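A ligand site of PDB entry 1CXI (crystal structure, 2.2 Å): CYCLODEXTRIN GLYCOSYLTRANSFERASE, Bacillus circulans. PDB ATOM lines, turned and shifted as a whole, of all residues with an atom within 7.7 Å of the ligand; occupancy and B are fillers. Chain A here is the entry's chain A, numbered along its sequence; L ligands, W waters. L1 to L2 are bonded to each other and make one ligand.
The backbone NH (N) of Ile 414 is in hydrogen-bond range of an oxygen (O3) of LIG L1 (2.9 Å). The backbone carbonyl oxygen (O) of Ile 414 sits at hydrogen-bond distance from an oxygen (O2) of LIG L1 (2.7 Å). O1 of LG2 L2 is in hydrogen-bond range of OE2 of Glu 411, 2.7 Å away. The backbone carbonyl oxygen (O) of Gly 446 is in hydrogen-bond range of an oxygen (O5) of LG2 L2, 2.7 Å away. O of Ser 445 is in hydrogen-bond range of O6 of LIG L1. NE1 of Trp 413 is in hydrogen-bond range of O5 of LIG L1.
N of Trp 413 sits at hydrogen-bond distance from OE2 of Glu 411, at 3.0 Å. The side-chain amino group (NZ) of Lys 304 is in salt-bridge range of the side-chain carboxylate (OE1) of Glu 411, at 2.8 Å. The guanidinium group of Arg 412 lies within hydrogen-bond range of the backbone carbonyl oxygen of Val 448 (3.0 Å). The backbone carbonyl oxygen (O) of Ile 420 sits at hydrogen-bond distance from the backbone NH (N) of Arg 412 (2.8 Å). The indole nitrogen (NE1) of Trp 413 sits at hydrogen-bond distance from the backbone carbonyl oxygen (O) of Ser 445 (2.9 Å). The backbone NH (N) of Ile 420 lies within hydrogen-bond range of the backbone carbonyl oxygen (O) of Trp 413 (2.9 Å).
O of Arg 412 lies close to O4 of LG2 L2 (3.3 Å). Hydrophobic or aromatic side chains that line the ligand: Trp 413 and Ile 414. Six residues have an atom within 4 Å of the ligand: Glu 411, Arg 412, Trp 413, Ile 414, Ser 445 and Gly 446. The nearest printed residue that does not touch the ligand is Val 448 (4.2 Å).
Water W2 bridges O of Glu 411 and O2 of LG2 L2. Water W1 lies within hydrogen-bond range of the side-chain hydroxyl (OH) of Tyr 301, the backbone carbonyl oxygen (O) of Ile 414 and an oxygen (O2) of LIG L1.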
ATOM      1  N   TYR A 301       2.349  26.021 -13.365  1.00  0.00           N
ATOM      2  CA  TYR A 301       0.958  25.818 -12.994  1.00  0.00           C
ATOM      3  C   TYR A 301       0.650  26.505 -11.666  1.00  0.00           C
ATOM      4  O   TYR A 301      -0.467  26.945 -11.425  1.00  0.00           O
ATOM      5  CB  TYR A 301       0.653  24.309 -12.918  1.00  0.00           C
ATOM      6  CG  TYR A 301       0.816  23.623 -14.250  1.00  0.00           C
ATOM      7  CD1 TYR A 301      -0.165  23.753 -15.233  1.00  0.00           C
ATOM      8  CD2 TYR A 301       1.941  22.858 -14.534  1.00  0.00           C
ATOM      9  CE1 TYR A 301      -0.018  23.153 -16.478  1.00  0.00           C
ATOM     10  CE2 TYR A 301       2.089  22.222 -15.771  1.00  0.00           C
ATOM     11  CZ  TYR A 301       1.109  22.388 -16.752  1.00  0.00           C
ATOM     12  OH  TYR A 301       1.253  21.810 -17.994  1.00  0.00           O
ATOM     13  N   LYS A 304       0.475  30.205 -12.294  1.00  0.00           N
ATOM     14  CA  LYS A 304      -0.828  30.459 -12.911  1.00  0.00           C
ATOM     15  C   LYS A 304      -1.969  30.430 -11.911  1.00  0.00           C
ATOM     16  O   LYS A 304      -2.866  31.271 -11.970  1.00  0.00           O
ATOM     17  CB  LYS A 304      -1.109  29.466 -14.033  1.00  0.00           C
ATOM     18  CG  LYS A 304      -2.592  29.384 -14.371  1.00  0.00           C
ATOM     19  CD  LYS A 304      -2.788  28.508 -15.586  1.00  0.00           C
ATOM     20  CE  LYS A 304      -4.101  27.775 -15.540  1.00  0.00           C
ATOM     21  NZ  LYS A 304      -4.987  28.031 -16.727  1.00  0.00           N
ATOM     22  N   GLN A 410      -4.468  36.819 -18.703  1.00  0.00           N
ATOM     23  CA  GLN A 410      -4.942  35.528 -19.188  1.00  0.00           C
ATOM     24  C   GLN A 410      -3.868  34.566 -19.681  1.00  0.00           C
ATOM     25  O   GLN A 410      -3.074  34.914 -20.541  1.00  0.00           O
ATOM     26  CB  GLN A 410      -6.006  35.666 -20.273  1.00  0.00           C
ATOM     27  CG  GLN A 410      -6.470  34.307 -20.734  1.00  0.00           C
ATOM     28  CD  GLN A 410      -7.441  34.355 -21.864  1.00  0.00           C
ATOM     29  OE1 GLN A 410      -7.990  33.329 -22.264  1.00  0.00           O
ATOM     30  NE2 GLN A 410      -7.678  35.547 -22.396  1.00  0.00           N
ATOM     31  N   GLU A 411      -3.884  33.334 -19.194  1.00  0.00           N
ATOM     32  CA  GLU A 411      -2.929  32.322 -19.627  1.00  0.00           C
ATOM     33  C   GLU A 411      -3.298  31.903 -21.055  1.00  0.00           C
ATOM     34  O   GLU A 411      -4.442  31.553 -21.326  1.00  0.00           O
ATOM     35  CB  GLU A 411      -2.969  31.119 -18.662  1.00  0.00           C
ATOM     36  CG  GLU A 411      -2.091  29.934 -19.087  1.00  0.00           C
ATOM     37  CD  GLU A 411      -2.884  28.911 -19.883  1.00  0.00           C
ATOM     38  OE1 GLU A 411      -3.843  28.350 -19.311  1.00  0.00           O
ATOM     39  OE2 GLU A 411      -2.573  28.687 -21.071  1.00  0.00           O
ATOM     40  N   ARG A 412      -2.324  31.955 -21.965  1.00  0.00           N
ATOM     41  CA  ARG A 412      -2.533  31.551 -23.359  1.00  0.00           C
ATOM     42  C   ARG A 412      -1.782  30.270 -23.766  1.00  0.00           C
ATOM     43  O   ARG A 412      -2.170  29.566 -24.697  1.00  0.00           O
ATOM     44  CB  ARG A 412      -2.253  32.719 -24.312  1.00  0.00           C
ATOM     45  CG  ARG A 412      -2.789  34.036 -23.754  1.00  0.00           C
ATOM     46  CD  ARG A 412      -3.857  34.749 -24.579  1.00  0.00           C
ATOM     47  NE  ARG A 412      -4.969  33.905 -24.966  1.00  0.00           N
ATOM     48  CZ  ARG A 412      -6.080  34.343 -25.562  1.00  0.00           C
ATOM     49  NH1 ARG A 412      -6.287  35.626 -25.819  1.00  0.00           N
ATOM     50  NH2 ARG A 412      -7.031  33.478 -25.898  1.00  0.00           N
ATOM     51  N   TRP A 413      -0.715  29.929 -23.028  1.00  0.00           N
ATOM     52  CA  TRP A 413       0.051  28.711 -23.302  1.00  0.00           C
ATOM     53  C   TRP A 413       0.780  28.339 -22.015  1.00  0.00           C
ATOM     54  O   TRP A 413       1.290  29.200 -21.299  1.00  0.00           O
ATOM     55  CB  TRP A 413       1.047  28.964 -24.433  1.00  0.00           C
ATOM     56  CG  TRP A 413       1.409  27.753 -25.277  1.00  0.00           C
ATOM     57  CD1 TRP A 413       0.908  27.425 -26.513  1.00  0.00           C
ATOM     58  CD2 TRP A 413       2.415  26.772 -24.987  1.00  0.00           C
ATOM     59  NE1 TRP A 413       1.533  26.288 -26.998  1.00  0.00           N
ATOM     60  CE2 TRP A 413       2.453  25.863 -26.078  1.00  0.00           C
ATOM     61  CE3 TRP A 413       3.298  26.564 -23.907  1.00  0.00           C
ATOM     62  CZ2 TRP A 413       3.312  24.781 -26.111  1.00  0.00           C
ATOM     63  CZ3 TRP A 413       4.137  25.458 -23.940  1.00  0.00           C
ATOM     64  CH2 TRP A 413       4.145  24.592 -25.045  1.00  0.00           C
ATOM     65  N   ILE A 414       0.826  27.050 -21.690  1.00  0.00           N
ATOM     66  CA  ILE A 414       1.527  26.679 -20.460  1.00  0.00           C
ATOM     67  C   ILE A 414       1.987  25.214 -20.384  1.00  0.00           C
ATOM     68  O   ILE A 414       1.324  24.332 -20.893  1.00  0.00           O
ATOM     69  CB  ILE A 414       0.601  26.945 -19.263  1.00  0.00           C
ATOM     70  CG1 ILE A 414       1.338  26.800 -17.932  1.00  0.00           C
ATOM     71  CG2 ILE A 414      -0.576  26.014 -19.316  1.00  0.00           C
ATOM     72  CD1 ILE A 414       0.450  26.955 -16.716  1.00  0.00           C
ATOM     73  N   ASN A 415       3.126  24.992 -19.736  1.00  0.00           N
ATOM     74  CA  ASN A 415       3.650  23.676 -19.385  1.00  0.00           C
ATOM     75  C   ASN A 415       4.444  23.823 -18.071  1.00  0.00           C
ATOM     76  O   ASN A 415       4.335  24.867 -17.427  1.00  0.00           O
ATOM     77  CB  ASN A 415       4.317  22.898 -20.537  1.00  0.00           C
ATOM     78  CG  ASN A 415       5.664  23.421 -20.912  1.00  0.00           C
ATOM     79  OD1 ASN A 415       6.268  24.212 -20.201  1.00  0.00           O
ATOM     80  ND2 ASN A 415       6.166  22.982 -22.074  1.00  0.00           N
ATOM     81  N   ASN A 416       5.171  22.807 -17.622  1.00  0.00           N
ATOM     82  CA  ASN A 416       5.878  22.938 -16.340  1.00  0.00           C
ATOM     83  C   ASN A 416       6.771  24.152 -16.288  1.00  0.00           C
ATOM     84  O   ASN A 416       6.936  24.753 -15.229  1.00  0.00           O
ATOM     85  CB  ASN A 416       6.849  21.766 -16.139  1.00  0.00           C
ATOM     86  CG  ASN A 416       6.165  20.481 -15.735  1.00  0.00           C
ATOM     87  OD1 ASN A 416       6.783  19.426 -15.709  1.00  0.00           O
ATOM     88  ND2 ASN A 416       4.902  20.572 -15.399  1.00  0.00           N
ATOM     89  N   VAL A 418       7.050  26.662 -19.069  1.00  0.00           N
ATOM     90  CA  VAL A 418       6.689  27.813 -19.892  1.00  0.00           C
ATOM     91  C   VAL A 418       5.356  28.429 -19.515  1.00  0.00           C
ATOM     92  O   VAL A 418       4.391  27.716 -19.264  1.00  0.00           O
ATOM     93  CB  VAL A 418       6.572  27.423 -21.387  1.00  0.00           C
ATOM     94  CG1 VAL A 418       6.135  28.634 -22.218  1.00  0.00           C
ATOM     95  CG2 VAL A 418       7.882  26.862 -21.919  1.00  0.00           C
ATOM     96  N   ILE A 420       2.897  31.638 -21.064  1.00  0.00           N
ATOM     97  CA  ILE A 420       2.682  32.741 -21.977  1.00  0.00           C
ATOM     98  C   ILE A 420       1.362  33.329 -21.502  1.00  0.00           C
ATOM     99  O   ILE A 420       0.350  32.633 -21.437  1.00  0.00           O
ATOM    100  CB  ILE A 420       2.622  32.303 -23.460  1.00  0.00           C
ATOM    101  CG1 ILE A 420       3.887  31.520 -23.821  1.00  0.00           C
ATOM    102  CG2 ILE A 420       2.438  33.537 -24.398  1.00  0.00           C
ATOM    103  CD1 ILE A 420       3.994  31.191 -25.306  1.00  0.00           C
ATOM    104  N   SER A 443       8.966  24.275 -27.820  1.00  0.00           N
ATOM    105  CA  SER A 443       8.398  24.456 -29.138  1.00  0.00           C
ATOM    106  C   SER A 443       6.970  24.978 -28.968  1.00  0.00           C
ATOM    107  O   SER A 443       6.105  24.290 -28.424  1.00  0.00           O
ATOM    108  CB  SER A 443       8.462  23.123 -29.907  1.00  0.00           C
ATOM    109  OG  SER A 443       7.625  23.150 -31.033  1.00  0.00           O
ATOM    110  N   ILE A 444       6.749  26.212 -29.378  1.00  0.00           N
ATOM    111  CA  ILE A 444       5.428  26.807 -29.225  1.00  0.00           C
ATOM    112  C   ILE A 444       4.466  26.833 -30.418  1.00  0.00           C
ATOM    113  O   ILE A 444       4.619  27.594 -31.384  1.00  0.00           O
ATOM    114  CB  ILE A 444       5.482  28.128 -28.429  1.00  0.00           C
ATOM    115  CG1 ILE A 444       5.922  27.809 -26.976  1.00  0.00           C
ATOM    116  CG2 ILE A 444       4.076  28.782 -28.414  1.00  0.00           C
ATOM    117  CD1 ILE A 444       7.267  28.259 -26.650  1.00  0.00           C
ATOM    118  N   SER A 445       3.450  25.965 -30.333  1.00  0.00           N
ATOM    119  CA  SER A 445       2.426  25.882 -31.376  1.00  0.00           C
ATOM    120  C   SER A 445       1.022  25.867 -30.770  1.00  0.00           C
ATOM    121  O   SER A 445       0.819  25.358 -29.682  1.00  0.00           O
ATOM    122  CB  SER A 445       2.648  24.659 -32.276  1.00  0.00           C
ATOM    123  OG  SER A 445       2.559  23.454 -31.538  1.00  0.00           O
ATOM    124  N   GLY A 446       0.051  26.446 -31.463  1.00  0.00           N
ATOM    125  CA  GLY A 446      -1.318  26.478 -30.948  1.00  0.00           C
ATOM    126  C   GLY A 446      -1.543  27.702 -30.068  1.00  0.00           C
ATOM    127  O   GLY A 446      -2.557  27.829 -29.425  1.00  0.00           O
ATOM    128  N   LEU A 447      -0.589  28.623 -30.042  1.00  0.00           N
ATOM    129  CA  LEU A 447      -0.755  29.823 -29.230  1.00  0.00           C
ATOM    130  C   LEU A 447      -1.734  30.759 -29.939  1.00  0.00           C
ATOM    131  O   LEU A 447      -1.534  31.120 -31.097  1.00  0.00           O
ATOM    132  CB  LEU A 447       0.574  30.558 -29.035  1.00  0.00           C
ATOM    133  CG  LEU A 447       0.520  31.968 -28.434  1.00  0.00           C
ATOM    134  CD1 LEU A 447       0.068  31.943 -26.985  1.00  0.00           C
ATOM    135  CD2 LEU A 447       1.857  32.677 -28.544  1.00  0.00           C
ATOM    136  N   VAL A 448      -2.761  31.166 -29.206  1.00  0.00           N
ATOM    137  CA  VAL A 448      -3.780  32.072 -29.721  1.00  0.00           C
ATOM    138  C   VAL A 448      -3.783  33.359 -28.851  1.00  0.00           C
ATOM    139  O   VAL A 448      -3.737  33.268 -27.612  1.00  0.00           O
ATOM    140  CB  VAL A 448      -5.153  31.353 -29.709  1.00  0.00           C
ATOM    141  CG1 VAL A 448      -6.300  32.343 -29.852  1.00  0.00           C
ATOM    142  CG2 VAL A 448      -5.203  30.283 -30.831  1.00  0.00           C
HETATM  143  C1  LIG L   1       0.234  22.692 -25.467  1.00  0.00           C
HETATM  144  C2  LIG L   1       0.305  23.610 -24.276  1.00  0.00           C
HETATM  145  C3  LIG L   1      -1.049  24.228 -24.007  1.00  0.00           C
HETATM  146  C4  LIG L   1      -1.552  24.878 -25.281  1.00  0.00           C
HETATM  147  C5  LIG L   1      -1.601  23.859 -26.420  1.00  0.00           C
HETATM  148  C6  LIG L   1      -2.077  24.582 -27.652  1.00  0.00           C
HETATM  149  O1  LIG L   1      -0.589  21.597 -25.267  1.00  0.00           O
HETATM  150  O2  LIG L   1       0.809  22.929 -23.125  1.00  0.00           O
HETATM  151  O3  LIG L   1      -0.988  25.168 -22.935  1.00  0.00           O
HETATM  152  O4  LIG L   1      -2.898  25.378 -25.172  1.00  0.00           O
HETATM  153  O5  LIG L   1      -0.243  23.446 -26.575  1.00  0.00           O
HETATM  154  O6  LIG L   1      -1.844  23.787 -28.818  1.00  0.00           O
HETATM  155  C1  LG2 L   2      -3.118  26.782 -25.147  1.00  0.00           C
HETATM  156  C2  LG2 L   2      -3.926  27.144 -23.917  1.00  0.00           C
HETATM  157  C3  LG2 L   2      -5.313  26.563 -24.014  1.00  0.00           C
HETATM  158  C4  LG2 L   2      -5.976  27.016 -25.314  1.00  0.00           C
HETATM  159  C5  LG2 L   2      -5.072  26.624 -26.476  1.00  0.00           C
HETATM  160  C6  LG2 L   2      -5.638  27.037 -27.809  1.00  0.00           C
HETATM  161  O1  LG2 L   2      -3.297  26.696 -22.724  1.00  0.00           O
HETATM  162  O2  LG2 L   2      -6.212  26.989 -22.981  1.00  0.00           O
HETATM  163  O3  LG2 L   2      -7.219  26.341 -25.443  1.00  0.00           O
HETATM  164  O4  LG2 L   2      -3.786  27.238 -26.315  1.00  0.00           O
HETATM  165  O5  LG2 L   2      -4.896  26.583 -28.948  1.00  0.00           O
HETATM  166  O   HOH W   1      -0.389  22.398 -20.035  1.00  0.00           O
HETATM  167  O   HOH W   2      -6.107  30.143 -23.030  1.00  0.00           O
HETATM  168  O   HOH W   3       2.324  20.734 -23.484  1.00  0.00           O
HETATM  169  O   HOH W   4      -3.666  29.918 -26.870  1.00  0.00           O
